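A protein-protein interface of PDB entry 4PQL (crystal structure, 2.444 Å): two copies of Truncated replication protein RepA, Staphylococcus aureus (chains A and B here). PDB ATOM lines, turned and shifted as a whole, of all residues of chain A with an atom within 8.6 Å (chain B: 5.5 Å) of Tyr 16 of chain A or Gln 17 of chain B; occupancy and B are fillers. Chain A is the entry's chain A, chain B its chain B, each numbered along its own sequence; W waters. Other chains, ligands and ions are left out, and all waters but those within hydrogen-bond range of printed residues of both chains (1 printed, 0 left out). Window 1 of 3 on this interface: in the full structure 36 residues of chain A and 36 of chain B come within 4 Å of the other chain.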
ATOM      1  N   LYS A  12      -4.014  20.637  28.990  1.00  0.00           N
ATOM      2  CA  LYS A  12      -4.898  19.989  29.957  1.00  0.00           C
ATOM      3  C   LYS A  12      -5.771  18.940  29.273  1.00  0.00           C
ATOM      4  O   LYS A  12      -6.149  17.940  29.879  1.00  0.00           O
ATOM      5  CB  LYS A  12      -5.772  21.027  30.661  1.00  0.00           C
ATOM      6  CG  LYS A  12      -5.304  21.367  32.053  1.00  0.00           C
ATOM      7  CD  LYS A  12      -6.059  22.546  32.614  1.00  0.00           C
ATOM      8  CE  LYS A  12      -5.129  23.409  33.438  1.00  0.00           C
ATOM      9  NZ  LYS A  12      -5.784  24.686  33.821  1.00  0.00           N
ATOM     10  N   GLU A  13      -6.052  19.166  27.994  1.00  0.00           N
ATOM     11  CA  GLU A  13      -6.934  18.306  27.221  1.00  0.00           C
ATOM     12  C   GLU A  13      -6.179  17.352  26.291  1.00  0.00           C
ATOM     13  O   GLU A  13      -6.646  17.059  25.194  1.00  0.00           O
ATOM     14  CB  GLU A  13      -7.922  19.154  26.413  1.00  0.00           C
ATOM     15  CG  GLU A  13      -8.932  19.908  27.264  1.00  0.00           C
ATOM     16  CD  GLU A  13      -9.880  18.976  28.017  1.00  0.00           C
ATOM     17  OE1 GLU A  13     -10.635  18.225  27.355  1.00  0.00           O
ATOM     18  OE2 GLU A  13      -9.873  18.989  29.269  1.00  0.00           O
ATOM     19  N   ARG A  14      -5.003  16.898  26.725  1.00  0.00           N
ATOM     20  CA  ARG A  14      -4.246  15.862  26.015  1.00  0.00           C
ATOM     21  C   ARG A  14      -4.323  14.561  26.808  1.00  0.00           C
ATOM     22  O   ARG A  14      -4.009  14.549  27.998  1.00  0.00           O
ATOM     23  CB  ARG A  14      -2.778  16.263  25.847  1.00  0.00           C
ATOM     24  CG  ARG A  14      -2.517  17.643  25.237  1.00  0.00           C
ATOM     25  CD  ARG A  14      -2.547  17.681  23.716  1.00  0.00           C
ATOM     26  NE  ARG A  14      -1.809  18.850  23.223  1.00  0.00           N
ATOM     27  CZ  ARG A  14      -1.493  19.075  21.947  1.00  0.00           C
ATOM     28  NH1 ARG A  14      -1.830  18.200  21.004  1.00  0.00           N
ATOM     29  NH2 ARG A  14      -0.820  20.171  21.612  1.00  0.00           N
ATOM     30  N   PHE A  15      -4.723  13.467  26.166  1.00  0.00           N
ATOM     31  CA  PHE A  15      -4.958  12.225  26.905  1.00  0.00           C
ATOM     32  C   PHE A  15      -4.301  10.997  26.296  1.00  0.00           C
ATOM     33  O   PHE A  15      -3.972  10.961  25.107  1.00  0.00           O
ATOM     34  CB  PHE A  15      -6.466  11.951  27.032  1.00  0.00           C
ATOM     35  CG  PHE A  15      -7.250  13.110  27.574  1.00  0.00           C
ATOM     36  CD1 PHE A  15      -7.935  13.959  26.719  1.00  0.00           C
ATOM     37  CD2 PHE A  15      -7.289  13.360  28.934  1.00  0.00           C
ATOM     38  CE1 PHE A  15      -8.650  15.040  27.214  1.00  0.00           C
ATOM     39  CE2 PHE A  15      -8.002  14.436  29.436  1.00  0.00           C
ATOM     40  CZ  PHE A  15      -8.685  15.274  28.574  1.00  0.00           C
ATOM     41  N   TYR A  16      -4.152   9.975  27.132  1.00  0.00           N
ATOM     42  CA  TYR A  16      -3.862   8.624  26.684  1.00  0.00           C
ATOM     43  C   TYR A  16      -5.173   7.861  26.775  1.00  0.00           C
ATOM     44  O   TYR A  16      -5.844   7.893  27.807  1.00  0.00           O
ATOM     45  CB  TYR A  16      -2.777   7.966  27.542  1.00  0.00           C
ATOM     46  CG  TYR A  16      -1.393   8.537  27.353  1.00  0.00           C
ATOM     47  CD1 TYR A  16      -0.602   8.860  28.443  1.00  0.00           C
ATOM     48  CD2 TYR A  16      -0.865   8.726  26.081  1.00  0.00           C
ATOM     49  CE1 TYR A  16       0.672   9.386  28.272  1.00  0.00           C
ATOM     50  CE2 TYR A  16       0.409   9.250  25.898  1.00  0.00           C
ATOM     51  CZ  TYR A  16       1.173   9.577  26.998  1.00  0.00           C
ATOM     52  OH  TYR A  16       2.440  10.096  26.830  1.00  0.00           O
ATOM     53  N   GLN A  17      -5.554   7.206  25.685  1.00  0.00           N
ATOM     54  CA  GLN A  17      -6.877   6.611  25.593  1.00  0.00           C
ATOM     55  C   GLN A  17      -6.842   5.106  25.715  1.00  0.00           C
ATOM     56  O   GLN A  17      -6.247   4.421  24.888  1.00  0.00           O
ATOM     57  CB  GLN A  17      -7.537   7.002  24.282  1.00  0.00           C
ATOM     58  CG  GLN A  17      -7.613   8.486  24.103  1.00  0.00           C
ATOM     59  CD  GLN A  17      -8.275   8.878  22.812  1.00  0.00           C
ATOM     60  OE1 GLN A  17      -9.262   9.619  22.816  1.00  0.00           O
ATOM     61  NE2 GLN A  17      -7.740   8.392  21.694  1.00  0.00           N
ATOM     62  N   ILE A  18      -7.508   4.606  26.751  1.00  0.00           N
ATOM     63  CA  ILE A  18      -7.657   3.184  26.974  1.00  0.00           C
ATOM     64  C   ILE A  18      -9.040   2.787  26.501  1.00  0.00           C
ATOM     65  O   ILE A  18     -10.020   3.386  26.917  1.00  0.00           O
ATOM     66  CB  ILE A  18      -7.505   2.805  28.460  1.00  0.00           C
ATOM     67  CG1 ILE A  18      -6.206   3.351  29.041  1.00  0.00           C
ATOM     68  CG2 ILE A  18      -7.593   1.288  28.642  1.00  0.00           C
ATOM     69  CD1 ILE A  18      -6.086   3.127  30.519  1.00  0.00           C
ATOM     70  N   PRO A  19      -9.120   1.802  25.595  1.00  0.00           N
ATOM     71  CA  PRO A  19     -10.417   1.356  25.079  1.00  0.00           C
ATOM     72  C   PRO A  19     -11.312   0.825  26.195  1.00  0.00           C
ATOM     73  O   PRO A  19     -10.830   0.072  27.045  1.00  0.00           O
ATOM     74  CB  PRO A  19     -10.043   0.244  24.101  1.00  0.00           C
ATOM     75  CG  PRO A  19      -8.624   0.507  23.737  1.00  0.00           C
ATOM     76  CD  PRO A  19      -7.997   1.095  24.956  1.00  0.00           C
ATOM     77  N   LYS A  20     -12.584   1.207  26.200  1.00  0.00           N
ATOM     78  CA  LYS A  20     -13.485   0.794  27.277  1.00  0.00           C
ATOM     79  C   LYS A  20     -13.688  -0.722  27.317  1.00  0.00           C
ATOM     80  O   LYS A  20     -13.886  -1.298  28.384  1.00  0.00           O
ATOM     81  CB  LYS A  20     -14.835   1.499  27.143  1.00  0.00           C
ATOM     82  CG  LYS A  20     -14.822   2.956  27.619  1.00  0.00           C
ATOM     83  CD  LYS A  20     -16.183   3.589  27.462  1.00  0.00           C
ATOM     84  CE  LYS A  20     -16.238   4.998  28.040  1.00  0.00           C
ATOM     85  NZ  LYS A  20     -17.625   5.312  28.478  1.00  0.00           N
ATOM     86  N   PHE A  23     -12.166  -3.223  29.787  1.00  0.00           N
ATOM     87  CA  PHE A  23     -12.735  -3.393  31.117  1.00  0.00           C
ATOM     88  C   PHE A  23     -13.978  -4.268  31.125  1.00  0.00           C
ATOM     89  O   PHE A  23     -14.456  -4.637  32.189  1.00  0.00           O
ATOM     90  CB  PHE A  23     -13.038  -2.023  31.735  1.00  0.00           C
ATOM     91  CG  PHE A  23     -11.818  -1.167  31.895  1.00  0.00           C
ATOM     92  CD1 PHE A  23     -11.322  -0.428  30.834  1.00  0.00           C
ATOM     93  CD2 PHE A  23     -11.165  -1.111  33.108  1.00  0.00           C
ATOM     94  CE1 PHE A  23     -10.184   0.337  30.977  1.00  0.00           C
ATOM     95  CE2 PHE A  23     -10.041  -0.342  33.264  1.00  0.00           C
ATOM     96  CZ  PHE A  23      -9.545   0.388  32.197  1.00  0.00           C
ATOM     97  N   LYS A  36      -2.642  -2.026  29.763  1.00  0.00           N
ATOM     98  CA  LYS A  36      -3.668  -1.121  29.259  1.00  0.00           C
ATOM     99  C   LYS A  36      -3.124   0.275  28.993  1.00  0.00           C
ATOM    100  O   LYS A  36      -3.347   0.867  27.917  1.00  0.00           O
ATOM    101  CB  LYS A  36      -4.833  -1.043  30.252  1.00  0.00           C
ATOM    102  CG  LYS A  36      -5.517  -2.371  30.469  1.00  0.00           C
ATOM    103  CD  LYS A  36      -6.840  -2.218  31.194  1.00  0.00           C
ATOM    104  CE  LYS A  36      -6.968  -3.251  32.303  1.00  0.00           C
ATOM    105  NZ  LYS A  36      -8.372  -3.330  32.793  1.00  0.00           N
ATOM    106  N   ILE A  37      -2.349   0.772  29.948  1.00  0.00           N
ATOM    107  CA  ILE A  37      -1.762   2.096  29.802  1.00  0.00           C
ATOM    108  C   ILE A  37      -0.747   2.122  28.649  1.00  0.00           C
ATOM    109  O   ILE A  37      -0.745   3.050  27.827  1.00  0.00           O
ATOM    110  CB  ILE A  37      -1.098   2.530  31.127  1.00  0.00           C
ATOM    111  CG1 ILE A  37      -2.177   2.792  32.180  1.00  0.00           C
ATOM    112  CG2 ILE A  37      -0.248   3.774  30.945  1.00  0.00           C
ATOM    113  CD1 ILE A  37      -1.662   2.823  33.594  1.00  0.00           C
ATOM    114  N   ALA A  38       0.072   1.076  28.552  1.00  0.00           N
ATOM    115  CA  ALA A  38       1.066   0.979  27.490  1.00  0.00           C
ATOM    116  C   ALA A  38       0.381   0.918  26.134  1.00  0.00           C
ATOM    117  O   ALA A  38       0.840   1.542  25.173  1.00  0.00           O
ATOM    118  CB  ALA A  38       1.966  -0.235  27.690  1.00  0.00           C
ATOM    119  N   TYR A  39      -0.752   0.217  26.071  1.00  0.00           N
ATOM    120  CA  TYR A  39      -1.509   0.160  24.823  1.00  0.00           C
ATOM    121  C   TYR A  39      -1.956   1.577  24.410  1.00  0.00           C
ATOM    122  O   TYR A  39      -1.796   1.978  23.238  1.00  0.00           O
ATOM    123  CB  TYR A  39      -2.729  -0.764  24.973  1.00  0.00           C
ATOM    124  CG  TYR A  39      -3.596  -0.819  23.732  1.00  0.00           C
ATOM    125  CD1 TYR A  39      -3.428  -1.834  22.790  1.00  0.00           C
ATOM    126  CD2 TYR A  39      -4.558   0.154  23.481  1.00  0.00           C
ATOM    127  CE1 TYR A  39      -4.208  -1.880  21.642  1.00  0.00           C
ATOM    128  CE2 TYR A  39      -5.329   0.121  22.340  1.00  0.00           C
ATOM    129  CZ  TYR A  39      -5.153  -0.901  21.427  1.00  0.00           C
ATOM    130  OH  TYR A  39      -5.927  -0.936  20.296  1.00  0.00           O
ATOM    131  N   ALA A  40      -2.438   2.352  25.384  1.00  0.00           N
ATOM    132  CA  ALA A  40      -2.886   3.722  25.110  1.00  0.00           C
ATOM    133  C   ALA A  40      -1.746   4.619  24.606  1.00  0.00           C
ATOM    134  O   ALA A  40      -1.869   5.378  23.594  1.00  0.00           O
ATOM    135  CB  ALA A  40      -3.505   4.319  26.369  1.00  0.00           C
ATOM    136  N   ILE A  41      -0.596   4.447  25.245  1.00  0.00           N
ATOM    137  CA  ILE A  41       0.579   5.235  24.899  1.00  0.00           C
ATOM    138  C   ILE A  41       1.044   4.916  23.481  1.00  0.00           C
ATOM    139  O   ILE A  41       1.333   5.831  22.681  1.00  0.00           O
ATOM    140  CB  ILE A  41       1.732   5.001  25.903  1.00  0.00           C
ATOM    141  CG1 ILE A  41       1.358   5.560  27.280  1.00  0.00           C
ATOM    142  CG2 ILE A  41       3.001   5.670  25.428  1.00  0.00           C
ATOM    143  CD1 ILE A  41       2.300   5.148  28.400  1.00  0.00           C
ATOM    144  N   LEU A  42       1.047   3.636  23.139  1.00  0.00           N
ATOM    145  CA  LEU A  42       1.439   3.243  21.797  1.00  0.00           C
ATOM    146  C   LEU A  42       0.462   3.789  20.751  1.00  0.00           C
ATOM    147  O   LEU A  42       0.863   4.143  19.637  1.00  0.00           O
ATOM    148  CB  LEU A  42       1.555   1.718  21.726  1.00  0.00           C
ATOM    149  CG  LEU A  42       2.787   1.204  22.488  1.00  0.00           C
ATOM    150  CD1 LEU A  42       2.805  -0.312  22.577  1.00  0.00           C
ATOM    151  CD2 LEU A  42       4.071   1.721  21.828  1.00  0.00           C
ATOM    152  N   ARG A  43      -0.812   3.890  21.097  1.00  0.00           N
ATOM    153  CA  ARG A  43      -1.770   4.419  20.123  1.00  0.00           C
ATOM    154  C   ARG A  43      -1.478   5.906  19.742  1.00  0.00           C
ATOM    155  O   ARG A  43      -1.433   6.348  18.514  1.00  0.00           O
ATOM    156  CB  ARG A  43      -3.159   4.201  20.736  1.00  0.00           C
ATOM    157  CG  ARG A  43      -4.360   4.441  19.875  1.00  0.00           C
ATOM    158  CD  ARG A  43      -5.632   4.327  20.706  1.00  0.00           C
ATOM    159  NE  ARG A  43      -6.702   3.852  19.840  1.00  0.00           N
ATOM    160  CZ  ARG A  43      -7.503   4.632  19.132  1.00  0.00           C
ATOM    161  NH1 ARG A  43      -8.427   4.082  18.348  1.00  0.00           N
ATOM    162  NH2 ARG A  43      -7.367   5.949  19.193  1.00  0.00           N
ATOM    163  N   ASP A  44      -1.097   6.655  20.778  1.00  0.00           N
ATOM    164  CA  ASP A  44      -0.709   8.051  20.530  1.00  0.00           C
ATOM    165  C   ASP A  44       0.575   8.021  19.638  1.00  0.00           C
ATOM    166  O   ASP A  44       0.799   8.827  18.636  1.00  0.00           O
ATOM    167  CB  ASP A  44      -0.506   8.733  21.896  1.00  0.00           C
ATOM    168  CG  ASP A  44      -0.054  10.167  21.797  1.00  0.00           C
ATOM    169  OD1 ASP A  44      -0.900  11.043  21.502  1.00  0.00           O
ATOM    170  OD2 ASP A  44       1.137  10.429  22.062  1.00  0.00           O
ATOM    171  N   ARG A  45       1.379   6.988  19.879  1.00  0.00           N
ATOM    172  CA  ARG A  45       2.581   6.944  19.079  1.00  0.00           C
ATOM    173  C   ARG A  45       2.191   6.620  17.638  1.00  0.00           C
ATOM    174  O   ARG A  45       2.989   6.862  16.731  1.00  0.00           O
ATOM    175  CB  ARG A  45       3.559   5.890  19.613  1.00  0.00           C
ATOM    176  CG  ARG A  45       4.322   6.315  20.852  1.00  0.00           C
ATOM    177  CD  ARG A  45       5.694   6.820  20.494  1.00  0.00           C
ATOM    178  NE  ARG A  45       6.231   7.677  21.545  1.00  0.00           N
ATOM    179  CZ  ARG A  45       7.397   8.302  21.468  1.00  0.00           C
ATOM    180  NH1 ARG A  45       8.149   8.163  20.385  1.00  0.00           N
ATOM    181  NH2 ARG A  45       7.810   9.064  22.471  1.00  0.00           N
ATOM    182  N   ILE A  73       9.868   5.020  26.117  1.00  0.00           N
ATOM    183  CA  ILE A  73       8.516   5.458  25.815  1.00  0.00           C
ATOM    184  C   ILE A  73       7.539   5.077  26.913  1.00  0.00           C
ATOM    185  O   ILE A  73       6.687   5.878  27.296  1.00  0.00           O
ATOM    186  CB  ILE A  73       8.030   4.846  24.468  1.00  0.00           C
ATOM    187  CG1 ILE A  73       8.829   5.413  23.291  1.00  0.00           C
ATOM    188  CG2 ILE A  73       6.548   5.100  24.255  1.00  0.00           C
ATOM    189  CD1 ILE A  73       8.610   4.675  21.976  1.00  0.00           C
ATOM    190  N   LEU A  74       7.686   3.861  27.432  1.00  0.00           N
ATOM    191  CA  LEU A  74       6.758   3.318  28.418  1.00  0.00           C
ATOM    192  C   LEU A  74       7.202   3.533  29.866  1.00  0.00           C
ATOM    193  O   LEU A  74       6.447   3.242  30.798  1.00  0.00           O
ATOM    194  CB  LEU A  74       6.576   1.816  28.170  1.00  0.00           C
ATOM    195  CG  LEU A  74       6.060   1.397  26.793  1.00  0.00           C
ATOM    196  CD1 LEU A  74       5.931  -0.121  26.724  1.00  0.00           C
ATOM    197  CD2 LEU A  74       4.731   2.065  26.496  1.00  0.00           C
ATOM    198  N   PHE B  15     -13.383   5.319  24.810  1.00  0.00           N
ATOM    199  CA  PHE B  15     -12.190   5.260  25.655  1.00  0.00           C
ATOM    200  C   PHE B  15     -12.367   5.870  27.045  1.00  0.00           C
ATOM    201  O   PHE B  15     -13.302   6.630  27.307  1.00  0.00           O
ATOM    202  CB  PHE B  15     -11.013   5.979  24.991  1.00  0.00           C
ATOM    203  CG  PHE B  15     -10.773   5.578  23.569  1.00  0.00           C
ATOM    204  CD1 PHE B  15     -11.237   6.376  22.528  1.00  0.00           C
ATOM    205  CD2 PHE B  15     -10.098   4.403  23.262  1.00  0.00           C
ATOM    206  CE1 PHE B  15     -11.022   6.015  21.209  1.00  0.00           C
ATOM    207  CE2 PHE B  15      -9.878   4.038  21.945  1.00  0.00           C
ATOM    208  CZ  PHE B  15     -10.342   4.844  20.915  1.00  0.00           C
ATOM    209  N   TYR B  16     -11.462   5.496  27.941  1.00  0.00           N
ATOM    210  CA  TYR B  16     -11.260   6.210  29.191  1.00  0.00           C
ATOM    211  C   TYR B  16      -9.994   7.026  29.023  1.00  0.00           C
ATOM    212  O   TYR B  16      -8.975   6.509  28.545  1.00  0.00           O
ATOM    213  CB  TYR B  16     -11.151   5.259  30.372  1.00  0.00           C
ATOM    214  CG  TYR B  16     -12.453   4.576  30.687  1.00  0.00           C
ATOM    215  CD1 TYR B  16     -12.564   3.194  30.629  1.00  0.00           C
ATOM    216  CD2 TYR B  16     -13.580   5.313  31.025  1.00  0.00           C
ATOM    217  CE1 TYR B  16     -13.764   2.563  30.916  1.00  0.00           C
ATOM    218  CE2 TYR B  16     -14.784   4.689  31.309  1.00  0.00           C
ATOM    219  CZ  TYR B  16     -14.872   3.319  31.252  1.00  0.00           C
ATOM    220  OH  TYR B  16     -16.067   2.696  31.535  1.00  0.00           O
ATOM    221  N   GLN B  17     -10.074   8.316  29.321  1.00  0.00           N
ATOM    222  CA  GLN B  17      -8.977   9.210  28.992  1.00  0.00           C
ATOM    223  C   GLN B  17      -8.176   9.648  30.209  1.00  0.00           C
ATOM    224  O   GLN B  17      -8.710  10.275  31.118  1.00  0.00           O
ATOM    225  CB  GLN B  17      -9.511  10.413  28.240  1.00  0.00           C
ATOM    226  CG  GLN B  17     -10.281  10.028  26.997  1.00  0.00           C
ATOM    227  CD  GLN B  17     -10.813  11.230  26.249  1.00  0.00           C
ATOM    228  OE1 GLN B  17     -11.567  12.036  26.794  1.00  0.00           O
ATOM    229  NE2 GLN B  17     -10.401  11.369  24.996  1.00  0.00           N
ATOM    230  N   ILE B  18      -6.891   9.307  30.209  1.00  0.00           N
ATOM    231  CA  ILE B  18      -5.954   9.714  31.250  1.00  0.00           C
ATOM    232  C   ILE B  18      -5.126  10.881  30.752  1.00  0.00           C
ATOM    233  O   ILE B  18      -4.487  10.773  29.705  1.00  0.00           O
ATOM    234  CB  ILE B  18      -4.993   8.563  31.652  1.00  0.00           C
ATOM    235  CG1 ILE B  18      -5.777   7.294  32.030  1.00  0.00           C
ATOM    236  CG2 ILE B  18      -4.075   8.998  32.786  1.00  0.00           C
ATOM    237  CD1 ILE B  18      -4.888   6.090  32.300  1.00  0.00           C
ATOM    238  N   PRO B  19      -5.125  11.997  31.502  1.00  0.00           N
ATOM    239  CA  PRO B  19      -4.359  13.184  31.108  1.00  0.00           C
ATOM    240  C   PRO B  19      -2.876  12.870  31.006  1.00  0.00           C
ATOM    241  O   PRO B  19      -2.317  12.193  31.870  1.00  0.00           O
ATOM    242  CB  PRO B  19      -4.646  14.184  32.235  1.00  0.00           C
ATOM    243  CG  PRO B  19      -5.926  13.727  32.849  1.00  0.00           C
ATOM    244  CD  PRO B  19      -5.907  12.227  32.732  1.00  0.00           C
ATOM    245  N   LYS B  20      -2.240  13.352  29.951  1.00  0.00           N
ATOM    246  CA  LYS B  20      -0.843  13.029  29.727  1.00  0.00           C
ATOM    247  C   LYS B  20       0.059  13.557  30.839  1.00  0.00           C
ATOM    248  O   LYS B  20       1.091  12.958  31.140  1.00  0.00           O
ATOM    249  CB  LYS B  20      -0.390  13.577  28.382  1.00  0.00           C
ATOM    250  CG  LYS B  20      -0.846  12.751  27.199  1.00  0.00           C
ATOM    251  CD  LYS B  20      -0.346  13.360  25.907  1.00  0.00           C
ATOM    252  CE  LYS B  20      -0.670  12.496  24.705  1.00  0.00           C
ATOM    253  NZ  LYS B  20       0.347  12.721  23.645  1.00  0.00           N
ATOM    254  N   PHE B  23       1.733  11.577  33.600  1.00  0.00           N
ATOM    255  CA  PHE B  23       2.953  10.826  33.342  1.00  0.00           C
ATOM    256  C   PHE B  23       4.179  11.734  33.235  1.00  0.00           C
ATOM    257  O   PHE B  23       5.299  11.238  33.229  1.00  0.00           O
ATOM    258  CB  PHE B  23       2.804   9.978  32.074  1.00  0.00           C
ATOM    259  CG  PHE B  23       1.669   9.002  32.147  1.00  0.00           C
ATOM    260  CD1 PHE B  23       0.379   9.397  31.833  1.00  0.00           C
ATOM    261  CD2 PHE B  23       1.875   7.712  32.599  1.00  0.00           C
ATOM    262  CE1 PHE B  23      -0.678   8.510  31.918  1.00  0.00           C
ATOM    263  CE2 PHE B  23       0.816   6.822  32.692  1.00  0.00           C
ATOM    264  CZ  PHE B  23      -0.461   7.227  32.352  1.00  0.00           C
ATOM    265  N   TYR B  39      -9.529   8.020  37.818  1.00  0.00           N
ATOM    266  CA  TYR B  39      -9.765   9.406  37.422  1.00  0.00           C
ATOM    267  C   TYR B  39     -10.384   9.449  36.013  1.00  0.00           C
ATOM    268  O   TYR B  39     -11.396  10.141  35.776  1.00  0.00           O
ATOM    269  CB  TYR B  39      -8.446  10.214  37.479  1.00  0.00           C
ATOM    270  CG  TYR B  39      -8.569  11.652  37.018  1.00  0.00           C
ATOM    271  CD1 TYR B  39      -8.780  12.680  37.929  1.00  0.00           C
ATOM    272  CD2 TYR B  39      -8.502  11.980  35.667  1.00  0.00           C
ATOM    273  CE1 TYR B  39      -8.906  13.992  37.511  1.00  0.00           C
ATOM    274  CE2 TYR B  39      -8.636  13.291  35.239  1.00  0.00           C
ATOM    275  CZ  TYR B  39      -8.838  14.291  36.164  1.00  0.00           C
ATOM    276  OH  TYR B  39      -8.961  15.596  35.742  1.00  0.00           O
ATOM    277  N   ALA B  40      -9.840   8.640  35.103  1.00  0.00           N
ATOM    278  CA  ALA B  40     -10.351   8.610  33.722  1.00  0.00           C
ATOM    279  C   ALA B  40     -11.829   8.150  33.653  1.00  0.00           C
ATOM    280  O   ALA B  40     -12.684   8.711  32.905  1.00  0.00           O
ATOM    281  CB  ALA B  40      -9.464   7.703  32.865  1.00  0.00           C
ATOM    282  N   ARG B  43     -14.212  10.815  34.923  1.00  0.00           N
ATOM    283  CA  ARG B  43     -14.404  11.895  33.948  1.00  0.00           C
ATOM    284  C   ARG B  43     -15.518  11.554  32.913  1.00  0.00           C
ATOM    285  O   ARG B  43     -16.512  12.361  32.598  1.00  0.00           O
ATOM    286  CB  ARG B  43     -13.042  12.136  33.286  1.00  0.00           C
ATOM    287  CG  ARG B  43     -12.923  13.332  32.394  1.00  0.00           C
ATOM    288  CD  ARG B  43     -11.592  13.320  31.664  1.00  0.00           C
ATOM    289  NE  ARG B  43     -11.803  13.837  30.322  1.00  0.00           N
ATOM    290  CZ  ARG B  43     -11.669  15.116  30.005  1.00  0.00           C
ATOM    291  NH1 ARG B  43     -11.244  15.983  30.916  1.00  0.00           N
ATOM    292  NH2 ARG B  43     -11.893  15.507  28.761  1.00  0.00           N
ATOM    293  N   GLU B 125       7.388  14.553  23.509  1.00  0.00           N
ATOM    294  CA  GLU B 125       6.789  13.253  23.247  1.00  0.00           C
ATOM    295  C   GLU B 125       5.977  13.250  21.953  1.00  0.00           C
ATOM    296  O   GLU B 125       6.085  12.337  21.144  1.00  0.00           O
ATOM    297  CB  GLU B 125       5.901  12.855  24.433  1.00  0.00           C
ATOM    298  CG  GLU B 125       5.339  11.446  24.385  1.00  0.00           C
ATOM    299  CD  GLU B 125       3.838  11.409  24.119  1.00  0.00           C
ATOM    300  OE1 GLU B 125       3.147  12.425  24.362  1.00  0.00           O
ATOM    301  OE2 GLU B 125       3.349  10.354  23.671  1.00  0.00           O
HETATM  302  O   HOH W   1      -2.557  16.446  29.734  1.00  0.00           O
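Phe 15 of chain A touches Pro 19 of chain B, and with the chains exchanged Pro 19 of chain A touches Phe 15 of chain B.
Tyr 16 of chain A touches Lys 20 of chain B, and with the chains exchanged Lys 20 of chain A touches Tyr 16 of chain B.
Gln 17 of chain A touches its own counterpart, Gln 17 of chain B.
Of the 29 pairs that touch across the chains among the printed residues, 21 have their exchanged pair printed and touching as well.
Water W1 bridges the backbone carbonyl oxygen (O) of Arg 14 of chain A (3.0 Å) and the backbone NH (N) of Lys 20 of chain B (3.1 Å).
Printed residues of chain A that touch a printed residue of chain B: Glu 13, Arg 14, Phe 15, Tyr 16, Gln 17, Ile 18, Pro 19, Lys 20, Phe 23, Ile 37, Arg 43, Asp 44 and Arg 45.
Hydrophobic or aromatic side chains of chain A within 4 Å of the printed part of chain B: Phe 15, Tyr 16, Ile 18, Phe 23 and Ile 37.
Of the 11 printed residues of chain B, 9 touch a printed residue of chain A.
Among the printed residues, Asp or Glu carboxylates within 4 Å of a Lys or Arg side-chain nitrogen of the other chain: Glu 13 of chain A with Arg 43 of chain B (3.3 Å) and Asp 44 of chain A with Lys 20 of chain B (2.9 Å).
The side-chain amino group (NZ) of Lys 20 of chain B lies within salt-bridge range of the side-chain carboxylate (OE1) of Glu 125 of chain B, 2.9 Å away.
Pro 19 of chain B touches Phe 15 of chain A.
O of Phe 15 of chain A touches CE of Lys 20 of chain B, at 3.7 Å.
NH2 of Arg 43 of chain B touches CZ of Phe 15 of chain A (3.2 Å).
Gln 17 of chain B touches Tyr 16 of chain A.
Phe 15 of chain B touches Lys 20 of chain A.
Ile 37 of chain A touches Phe 23 of chain B.
CG of Glu 125 of chain B touches NH2 of Arg 45 of chain A, at 3.9 Å.
The side-chain carboxylate (OE1) of Glu 13 of chain A lies within salt-bridge range of the guanidinium group (NH2) of Arg 43 of chain B, 3.3 Å away.
The side-chain amide oxygen of Gln 17 of chain A lies within hydrogen-bond range of the side-chain amide nitrogen of Gln 17 of chain B, 3.0 Å away.
O of Ile 18 of chain A sits at hydrogen-bond distance from N of Tyr 16 of chain B (2.8 Å).
The side-chain carboxylate of Asp 44 of chain A lies close to the side-chain carboxylate of Glu 125 of chain B (2.7 Å).
The side-chain hydroxyl of Tyr 16 of chain A is in hydrogen-bond range of the side-chain carboxylate of Glu 125 of chain B (3.3 Å).
N of Lys 20 of chain B sits at hydrogen-bond distance from O of Arg 14 of chain A (2.9 Å).
The backbone NH (N) of Tyr 16 of chain A sits at hydrogen-bond distance from the backbone carbonyl oxygen (O) of Ile 18 of chain B (2.7 Å).
OD2 of Asp 44 of chain A lies within salt-bridge range of NZ of Lys 20 of chain B (2.9 Å).
Of chain B, only Tyr 16, Gln 17, Ile 18, Lys 20, Phe 23 and Glu 125 come within 4 Å of Tyr 16 of chain A.
Of the printed residues of chain A, Gln 17 of chain B touches Phe 15, Tyr 16 and Gln 17.
No residue of chain A comes within 4 Å of Ala 40 of chain B.
Of the printed residues of chain B, Arg 45 of chain A touches Glu 125 (3.9 Å).
Of the printed residues of chain A, Ile 18 of chain B touches Phe 15 (3.2 Å), Tyr 16 (2.7 Å) and Ile 18 (3.7 Å).
Of the printed residues of chain A, Arg 43 of chain B touches Glu 13 (3.3 Å) and Phe 15 (3.2 Å).
Ile 41 of chain A touches none of the printed residues of chain B.
The nearest residue of chain B that does not touch Tyr 16 of chain A is Pro 19 of chain B (4.9 Å).
The nearest residue of chain A that does not touch Gln 17 of chain B is Ile 18 of chain A (5.2 Å).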
